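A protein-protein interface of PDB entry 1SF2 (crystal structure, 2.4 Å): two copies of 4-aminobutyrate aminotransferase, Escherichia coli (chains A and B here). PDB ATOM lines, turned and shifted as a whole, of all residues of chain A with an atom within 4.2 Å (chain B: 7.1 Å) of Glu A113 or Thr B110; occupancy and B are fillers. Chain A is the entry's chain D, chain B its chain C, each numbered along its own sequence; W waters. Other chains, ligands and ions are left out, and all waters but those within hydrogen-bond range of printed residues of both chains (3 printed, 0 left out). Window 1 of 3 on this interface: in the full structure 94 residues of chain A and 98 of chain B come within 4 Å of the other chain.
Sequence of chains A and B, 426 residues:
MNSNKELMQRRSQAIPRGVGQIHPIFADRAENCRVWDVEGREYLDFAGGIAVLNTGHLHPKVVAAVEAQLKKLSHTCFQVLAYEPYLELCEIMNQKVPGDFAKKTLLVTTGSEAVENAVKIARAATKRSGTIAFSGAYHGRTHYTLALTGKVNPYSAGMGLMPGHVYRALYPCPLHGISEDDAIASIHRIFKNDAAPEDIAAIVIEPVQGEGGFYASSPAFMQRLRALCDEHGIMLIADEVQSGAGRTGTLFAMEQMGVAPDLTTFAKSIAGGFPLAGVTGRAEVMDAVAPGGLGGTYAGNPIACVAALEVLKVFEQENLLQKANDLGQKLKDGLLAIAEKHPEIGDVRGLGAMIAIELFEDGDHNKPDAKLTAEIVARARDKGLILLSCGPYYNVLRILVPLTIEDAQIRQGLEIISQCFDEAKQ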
ATOM      1  N   VAL A 108      10.779   1.975  -1.231  1.00  0.00           N
ATOM      2  CA  VAL A 108      10.815   3.293  -0.620  1.00  0.00           C
ATOM      3  C   VAL A 108      11.221   3.071   0.848  1.00  0.00           C
ATOM      4  O   VAL A 108      11.996   2.158   1.155  1.00  0.00           O
ATOM      5  CB  VAL A 108       9.455   3.990  -0.727  1.00  0.00           C
ATOM      6  CG1 VAL A 108       9.159   4.290  -2.185  1.00  0.00           C
ATOM      7  CG2 VAL A 108       8.361   3.114  -0.140  1.00  0.00           C
ATOM      8  N   THR A 109      10.718   3.881   1.771  1.00  0.00           N
ATOM      9  CA  THR A 109      11.121   3.673   3.154  1.00  0.00           C
ATOM     10  C   THR A 109       9.978   3.474   4.153  1.00  0.00           C
ATOM     11  O   THR A 109      10.096   2.661   5.060  1.00  0.00           O
ATOM     12  CB  THR A 109      12.019   4.820   3.625  1.00  0.00           C
ATOM     13  OG1 THR A 109      13.081   4.999   2.682  1.00  0.00           O
ATOM     14  CG2 THR A 109      12.596   4.513   5.006  1.00  0.00           C
ATOM     15  N   THR A 110       8.874   4.188   3.979  1.00  0.00           N
ATOM     16  CA  THR A 110       7.766   4.058   4.911  1.00  0.00           C
ATOM     17  C   THR A 110       6.500   3.639   4.201  1.00  0.00           C
ATOM     18  O   THR A 110       6.345   3.889   2.993  1.00  0.00           O
ATOM     19  CB  THR A 110       7.492   5.400   5.666  1.00  0.00           C
ATOM     20  OG1 THR A 110       7.075   6.404   4.727  1.00  0.00           O
ATOM     21  CG2 THR A 110       8.761   5.882   6.404  1.00  0.00           C
ATOM     22  N   GLY A 111       5.600   2.999   4.949  1.00  0.00           N
ATOM     23  CA  GLY A 111       4.333   2.560   4.387  1.00  0.00           C
ATOM     24  C   GLY A 111       3.549   3.708   3.766  1.00  0.00           C
ATOM     25  O   GLY A 111       2.847   3.530   2.767  1.00  0.00           O
ATOM     26  N   SER A 112       3.674   4.890   4.357  1.00  0.00           N
ATOM     27  CA  SER A 112       2.994   6.080   3.862  1.00  0.00           C
ATOM     28  C   SER A 112       3.530   6.396   2.480  1.00  0.00           C
ATOM     29  O   SER A 112       2.775   6.669   1.554  1.00  0.00           O
ATOM     30  CB  SER A 112       3.246   7.268   4.801  1.00  0.00           C
ATOM     31  OG  SER A 112       2.605   7.083   6.055  1.00  0.00           O
ATOM     32  N   GLU A 113       4.848   6.358   2.354  1.00  0.00           N
ATOM     33  CA  GLU A 113       5.495   6.630   1.085  1.00  0.00           C
ATOM     34  C   GLU A 113       5.073   5.555   0.082  1.00  0.00           C
ATOM     35  O   GLU A 113       4.904   5.842  -1.096  1.00  0.00           O
ATOM     36  CB  GLU A 113       7.020   6.591   1.213  1.00  0.00           C
ATOM     37  CG  GLU A 113       7.645   7.737   1.971  1.00  0.00           C
ATOM     38  CD  GLU A 113       9.147   7.741   1.812  1.00  0.00           C
ATOM     39  OE1 GLU A 113       9.782   6.674   1.957  1.00  0.00           O
ATOM     40  OE2 GLU A 113       9.700   8.813   1.542  1.00  0.00           O
ATOM     41  N   ALA A 114       4.922   4.314   0.547  1.00  0.00           N
ATOM     42  CA  ALA A 114       4.519   3.236  -0.349  1.00  0.00           C
ATOM     43  C   ALA A 114       3.149   3.535  -0.960  1.00  0.00           C
ATOM     44  O   ALA A 114       2.958   3.428  -2.174  1.00  0.00           O
ATOM     45  CB  ALA A 114       4.484   1.910   0.399  1.00  0.00           C
ATOM     46  N   VAL A 115       2.189   3.912  -0.128  1.00  0.00           N
ATOM     47  CA  VAL A 115       0.875   4.206  -0.662  1.00  0.00           C
ATOM     48  C   VAL A 115       0.963   5.428  -1.581  1.00  0.00           C
ATOM     49  O   VAL A 115       0.380   5.432  -2.672  1.00  0.00           O
ATOM     50  CB  VAL A 115      -0.136   4.439   0.466  1.00  0.00           C
ATOM     51  CG1 VAL A 115      -1.456   4.952  -0.110  1.00  0.00           C
ATOM     52  CG2 VAL A 115      -0.357   3.125   1.223  1.00  0.00           C
ATOM     53  N   GLU A 116       1.705   6.448  -1.158  1.00  0.00           N
ATOM     54  CA  GLU A 116       1.889   7.653  -1.972  1.00  0.00           C
ATOM     55  C   GLU A 116       2.295   7.284  -3.406  1.00  0.00           C
ATOM     56  O   GLU A 116       1.673   7.711  -4.380  1.00  0.00           O
ATOM     57  CB  GLU A 116       2.994   8.533  -1.376  1.00  0.00           C
ATOM     58  CG  GLU A 116       2.593   9.384  -0.186  1.00  0.00           C
ATOM     59  CD  GLU A 116       1.889  10.669  -0.594  1.00  0.00           C
ATOM     60  OE1 GLU A 116       1.925  11.040  -1.792  1.00  0.00           O
ATOM     61  OE2 GLU A 116       1.305  11.322   0.293  1.00  0.00           O
ATOM     62  N   ASN A 117       3.353   6.488  -3.519  1.00  0.00           N
ATOM     63  CA  ASN A 117       3.871   6.068  -4.812  1.00  0.00           C
ATOM     64  C   ASN A 117       2.924   5.150  -5.569  1.00  0.00           C
ATOM     65  O   ASN A 117       2.804   5.254  -6.787  1.00  0.00           O
ATOM     66  CB  ASN A 117       5.239   5.418  -4.624  1.00  0.00           C
ATOM     67  CG  ASN A 117       6.332   6.446  -4.377  1.00  0.00           C
ATOM     68  OD1 ASN A 117       6.759   7.142  -5.305  1.00  0.00           O
ATOM     69  ND2 ASN A 117       6.785   6.561  -3.121  1.00  0.00           N
ATOM     70  N   VAL B 108      10.680  11.779  12.428  1.00  0.00           N
ATOM     71  CA  VAL B 108       9.927  10.976  11.471  1.00  0.00           C
ATOM     72  C   VAL B 108      11.006  10.103  10.833  1.00  0.00           C
ATOM     73  O   VAL B 108      12.010   9.824  11.489  1.00  0.00           O
ATOM     74  CB  VAL B 108       9.190  11.851  10.424  1.00  0.00           C
ATOM     75  CG1 VAL B 108       8.100  12.676  11.119  1.00  0.00           C
ATOM     76  CG2 VAL B 108      10.169  12.760   9.695  1.00  0.00           C
ATOM     77  N   THR B 109      10.834   9.666   9.583  1.00  0.00           N
ATOM     78  CA  THR B 109      11.852   8.815   8.961  1.00  0.00           C
ATOM     79  C   THR B 109      12.546   9.392   7.730  1.00  0.00           C
ATOM     80  O   THR B 109      13.755   9.208   7.560  1.00  0.00           O
ATOM     81  CB  THR B 109      11.274   7.439   8.575  1.00  0.00           C
ATOM     82  OG1 THR B 109      10.604   6.861   9.709  1.00  0.00           O
ATOM     83  CG2 THR B 109      12.412   6.494   8.114  1.00  0.00           C
ATOM     84  N   THR B 110      11.797  10.084   6.868  1.00  0.00           N
ATOM     85  CA  THR B 110      12.380  10.656   5.650  1.00  0.00           C
ATOM     86  C   THR B 110      12.207  12.181   5.538  1.00  0.00           C
ATOM     87  O   THR B 110      11.294  12.775   6.135  1.00  0.00           O
ATOM     88  CB  THR B 110      11.773   9.983   4.367  1.00  0.00           C
ATOM     89  OG1 THR B 110      10.408  10.381   4.203  1.00  0.00           O
ATOM     90  CG2 THR B 110      11.799   8.462   4.489  1.00  0.00           C
ATOM     91  N   GLY B 111      13.095  12.809   4.771  1.00  0.00           N
ATOM     92  CA  GLY B 111      13.016  14.244   4.577  1.00  0.00           C
ATOM     93  C   GLY B 111      11.644  14.657   4.064  1.00  0.00           C
ATOM     94  O   GLY B 111      11.133  15.723   4.409  1.00  0.00           O
ATOM     95  N   SER B 112      11.046  13.820   3.224  1.00  0.00           N
ATOM     96  CA  SER B 112       9.721  14.123   2.707  1.00  0.00           C
ATOM     97  C   SER B 112       8.722  14.220   3.855  1.00  0.00           C
ATOM     98  O   SER B 112       7.911  15.151   3.913  1.00  0.00           O
ATOM     99  CB  SER B 112       9.262  13.031   1.746  1.00  0.00           C
ATOM    100  OG  SER B 112       9.979  13.103   0.532  1.00  0.00           O
ATOM    101  N   GLU B 113       8.763  13.233   4.747  1.00  0.00           N
ATOM    102  CA  GLU B 113       7.851  13.215   5.883  1.00  0.00           C
ATOM    103  C   GLU B 113       8.101  14.424   6.771  1.00  0.00           C
ATOM    104  O   GLU B 113       7.174  14.972   7.367  1.00  0.00           O
ATOM    105  CB  GLU B 113       8.030  11.938   6.712  1.00  0.00           C
ATOM    106  CG  GLU B 113       7.625  10.663   6.015  1.00  0.00           C
ATOM    107  CD  GLU B 113       7.678   9.474   6.948  1.00  0.00           C
ATOM    108  OE1 GLU B 113       8.630   9.394   7.746  1.00  0.00           O
ATOM    109  OE2 GLU B 113       6.781   8.613   6.889  1.00  0.00           O
ATOM    110  N   ALA B 114       9.360  14.833   6.857  1.00  0.00           N
ATOM    111  CA  ALA B 114       9.716  15.985   7.674  1.00  0.00           C
ATOM    112  C   ALA B 114       8.978  17.219   7.152  1.00  0.00           C
ATOM    113  O   ALA B 114       8.301  17.914   7.914  1.00  0.00           O
ATOM    114  CB  ALA B 114      11.215  16.207   7.643  1.00  0.00           C
ATOM    115  N   VAL B 115       9.086  17.488   5.855  1.00  0.00           N
ATOM    116  CA  VAL B 115       8.397  18.638   5.305  1.00  0.00           C
ATOM    117  C   VAL B 115       6.896  18.482   5.483  1.00  0.00           C
ATOM    118  O   VAL B 115       6.213  19.417   5.884  1.00  0.00           O
ATOM    119  CB  VAL B 115       8.731  18.836   3.818  1.00  0.00           C
ATOM    120  CG1 VAL B 115       7.965  20.052   3.278  1.00  0.00           C
ATOM    121  CG2 VAL B 115      10.258  19.015   3.655  1.00  0.00           C
ATOM    122  N   GLU B 116       6.381  17.297   5.194  1.00  0.00           N
ATOM    123  CA  GLU B 116       4.955  17.042   5.358  1.00  0.00           C
ATOM    124  C   GLU B 116       4.468  17.441   6.761  1.00  0.00           C
ATOM    125  O   GLU B 116       3.447  18.131   6.914  1.00  0.00           O
ATOM    126  CB  GLU B 116       4.655  15.554   5.122  1.00  0.00           C
ATOM    127  CG  GLU B 116       4.700  15.128   3.656  1.00  0.00           C
ATOM    128  CD  GLU B 116       3.339  15.237   2.991  1.00  0.00           C
ATOM    129  OE1 GLU B 116       2.393  15.758   3.634  1.00  0.00           O
ATOM    130  OE2 GLU B 116       3.218  14.796   1.825  1.00  0.00           O
ATOM    131  N   ASN B 117       5.201  17.001   7.780  1.00  0.00           N
ATOM    132  CA  ASN B 117       4.830  17.283   9.158  1.00  0.00           C
ATOM    133  C   ASN B 117       5.009  18.727   9.557  1.00  0.00           C
ATOM    134  O   ASN B 117       4.176  19.277  10.277  1.00  0.00           O
ATOM    135  CB  ASN B 117       5.600  16.362  10.091  1.00  0.00           C
ATOM    136  CG  ASN B 117       4.998  14.971  10.141  1.00  0.00           C
ATOM    137  OD1 ASN B 117       4.047  14.724  10.884  1.00  0.00           O
ATOM    138  ND2 ASN B 117       5.531  14.060   9.327  1.00  0.00           N
ATOM    139  N   ARG B 141       9.052  13.738  -2.642  1.00  0.00           N
ATOM    140  CA  ARG B 141       8.247  13.142  -3.693  1.00  0.00           C
ATOM    141  C   ARG B 141       6.889  12.581  -3.276  1.00  0.00           C
ATOM    142  O   ARG B 141       6.396  11.626  -3.880  1.00  0.00           O
ATOM    143  CB  ARG B 141       9.056  12.052  -4.413  1.00  0.00           C
ATOM    144  CG  ARG B 141      10.293  12.538  -5.183  1.00  0.00           C
ATOM    145  CD  ARG B 141      11.277  11.368  -5.368  1.00  0.00           C
ATOM    146  NE  ARG B 141      12.478  11.719  -6.129  1.00  0.00           N
ATOM    147  CZ  ARG B 141      12.540  11.808  -7.457  1.00  0.00           C
ATOM    148  NH1 ARG B 141      11.469  11.577  -8.197  1.00  0.00           N
ATOM    149  NH2 ARG B 141      13.688  12.112  -8.046  1.00  0.00           N
ATOM    150  N   THR B 142       6.292  13.148  -2.235  1.00  0.00           N
ATOM    151  CA  THR B 142       4.954  12.719  -1.835  1.00  0.00           C
ATOM    152  C   THR B 142       4.093  13.700  -2.618  1.00  0.00           C
ATOM    153  O   THR B 142       4.619  14.697  -3.129  1.00  0.00           O
ATOM    154  CB  THR B 142       4.684  12.893  -0.306  1.00  0.00           C
ATOM    155  OG1 THR B 142       4.989  14.236   0.093  1.00  0.00           O
ATOM    156  CG2 THR B 142       5.518  11.915   0.501  1.00  0.00           C
ATOM    157  N   VAL B 241      16.962  19.798   5.081  1.00  0.00           N
ATOM    158  CA  VAL B 241      17.249  18.399   4.853  1.00  0.00           C
ATOM    159  C   VAL B 241      18.602  18.204   4.155  1.00  0.00           C
ATOM    160  O   VAL B 241      19.362  17.301   4.507  1.00  0.00           O
ATOM    161  CB  VAL B 241      16.124  17.777   4.034  1.00  0.00           C
ATOM    162  CG1 VAL B 241      16.534  16.402   3.494  1.00  0.00           C
ATOM    163  CG2 VAL B 241      14.898  17.665   4.920  1.00  0.00           C
ATOM    164  N   PHE B 266      15.047  18.391   8.983  1.00  0.00           N
ATOM    165  CA  PHE B 266      16.372  17.834   8.807  1.00  0.00           C
ATOM    166  C   PHE B 266      16.266  16.353   8.500  1.00  0.00           C
ATOM    167  O   PHE B 266      15.286  15.693   8.876  1.00  0.00           O
ATOM    168  CB  PHE B 266      17.218  18.085  10.067  1.00  0.00           C
ATOM    169  CG  PHE B 266      16.635  17.508  11.326  1.00  0.00           C
ATOM    170  CD1 PHE B 266      16.832  16.167  11.656  1.00  0.00           C
ATOM    171  CD2 PHE B 266      15.905  18.308  12.197  1.00  0.00           C
ATOM    172  CE1 PHE B 266      16.314  15.633  12.836  1.00  0.00           C
ATOM    173  CE2 PHE B 266      15.382  17.783  13.378  1.00  0.00           C
ATOM    174  CZ  PHE B 266      15.589  16.443  13.700  1.00  0.00           C
ATOM    175  N   ALA B 267      17.277  15.847   7.804  1.00  0.00           N
ATOM    176  CA  ALA B 267      17.347  14.447   7.417  1.00  0.00           C
ATOM    177  C   ALA B 267      18.744  14.239   6.847  1.00  0.00           C
ATOM    178  O   ALA B 267      19.708  14.841   7.330  1.00  0.00           O
ATOM    179  CB  ALA B 267      16.290  14.134   6.356  1.00  0.00           C
ATOM    180  N   LYS B 268      18.837  13.406   5.811  1.00  0.00           N
ATOM    181  CA  LYS B 268      20.092  13.080   5.151  1.00  0.00           C
ATOM    182  C   LYS B 268      21.310  12.885   6.081  1.00  0.00           C
ATOM    183  O   LYS B 268      21.404  11.860   6.773  1.00  0.00           O
ATOM    184  CB  LYS B 268      20.402  14.114   4.057  1.00  0.00           C
ATOM    185  CG  LYS B 268      19.425  14.050   2.870  1.00  0.00           C
ATOM    186  CD  LYS B 268      19.949  14.737   1.610  1.00  0.00           C
ATOM    187  CE  LYS B 268      19.017  14.512   0.391  1.00  0.00           C
ATOM    188  NZ  LYS B 268      17.798  15.381   0.440  1.00  0.00           N
ATOM    189  N   PRO B 275      18.379   5.730   7.995  1.00  0.00           N
ATOM    190  CA  PRO B 275      17.052   6.346   7.852  1.00  0.00           C
ATOM    191  C   PRO B 275      16.437   7.088   9.043  1.00  0.00           C
ATOM    192  O   PRO B 275      15.786   6.491   9.905  1.00  0.00           O
ATOM    193  CB  PRO B 275      16.161   5.180   7.396  1.00  0.00           C
ATOM    194  CG  PRO B 275      17.124   4.069   7.029  1.00  0.00           C
ATOM    195  CD  PRO B 275      18.270   4.264   7.978  1.00  0.00           C
ATOM    196  N   LEU B 276      16.613   8.405   9.053  1.00  0.00           N
ATOM    197  CA  LEU B 276      16.068   9.236  10.109  1.00  0.00           C
ATOM    198  C   LEU B 276      15.866  10.647   9.595  1.00  0.00           C
ATOM    199  O   LEU B 276      16.652  11.138   8.782  1.00  0.00           O
ATOM    200  CB  LEU B 276      17.021   9.273  11.308  1.00  0.00           C
ATOM    201  CG  LEU B 276      16.615  10.179  12.477  1.00  0.00           C
ATOM    202  CD1 LEU B 276      15.455   9.555  13.247  1.00  0.00           C
ATOM    203  CD2 LEU B 276      17.779  10.341  13.398  1.00  0.00           C
ATOM    204  N   ALA B 277      14.807  11.286  10.080  1.00  0.00           N
ATOM    205  CA  ALA B 277      14.474  12.663   9.729  1.00  0.00           C
ATOM    206  C   ALA B 277      13.706  13.289  10.905  1.00  0.00           C
ATOM    207  O   ALA B 277      13.292  12.585  11.828  1.00  0.00           O
ATOM    208  CB  ALA B 277      13.619  12.697   8.462  1.00  0.00           C
ATOM    209  N   GLY B 278      13.515  14.604  10.865  1.00  0.00           N
ATOM    210  CA  GLY B 278      12.802  15.267  11.939  1.00  0.00           C
ATOM    211  C   GLY B 278      12.446  16.726  11.692  1.00  0.00           C
ATOM    212  O   GLY B 278      12.855  17.339  10.698  1.00  0.00           O
HETATM  213  O   HOH W   1       0.904  14.036   0.426  1.00  0.00           O
HETATM  214  O   HOH W   2       9.212  10.367  -0.578  1.00  0.00           O
HETATM  215  O   HOH W   3       4.272   9.711   7.218  1.00  0.00           O
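N of Thr B109 lies within hydrogen-bond range of OE1 of Glu B113, at 2.9 Å.
The backbone carbonyl oxygen of Thr B109 lies close to the backbone NH of Leu B276, at 3.3 Å.
The backbone NH (N) of Ala B277 is in hydrogen-bond range of the backbone carbonyl oxygen (O) of Thr B109 (3.4 Å).
The backbone NH (N) of Glu B113 sits close to the side-chain hydroxyl (OG1) of Thr B110.
The side-chain amide nitrogen (ND2) of Asn B117 sits at hydrogen-bond distance from the backbone carbonyl oxygen (O) of Glu B113 (2.7 Å).
O of Glu A113 is in hydrogen-bond range of ND2 of Asn A117, at 2.9 Å.
Glu A113 touches just one residue of chain B: Thr B110 (3.2 Å).
Of chain A, only Thr A109 (3.7 Å) and Glu A113 (3.2 Å) come within 4 Å of Thr B110.
Printed residues of chain B within 4 Å of Thr A110: Thr B109 (3.7 Å) and Glu B113 (3.1 Å).
Of the printed residues of chain B, Glu A116 touches Thr B142.
Printed residues of chain A within 4 Å of Thr B142: Glu A116 (3.5 Å).
The nearest printed residue of chain A that does not touch Thr B110 is Thr A110 (4.4 Å).
The nearest printed residue of chain A that does not touch Glu B113 is Ser A112 (4.3 Å).
The side-chain hydroxyl of Thr B110 is in hydrogen-bond range of the side-chain carboxylate of Glu A113, at 3.2 Å.
OE2 of Glu B113 sits at hydrogen-bond distance from OG1 of Thr A110, 3.1 Å away.
Water W2 bridges OE2 of Glu A113 (2.7 Å) and OG of Ser B112 (3.1 Å).
Water W1 bridges OE2 of Glu A116 (2.7 Å) and OE2 of Glu B116 (2.8 Å).
Water W3 bridges the side-chain carboxylate (OE2) of Glu B113 (2.8 Å) and the side-chain hydroxyl (OG) of Ser A112 (3.3 Å).
Among the printed residues, pairs that only touch across the chains: Glu A116 with Thr B142, Thr A110 with Thr B109, Thr A109 with Thr B109 and Thr A109 with Thr B110.
Thr A109 touches its own counterpart, Thr B109.
Thr A109 touches Thr B110, and with the chains exchanged Thr A110 touches Thr B109.
Thr A110 touches Glu B113, and with the chains exchanged Glu A113 touches Thr B110.
Positions printed for both chains: 108, 109, 110, 111, 112, 113, 114, 115, 116 and 117.
Among the printed residues, no Asp or Glu carboxylate lies within 4 Å of a Lys or Arg side-chain nitrogen of the other chain.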
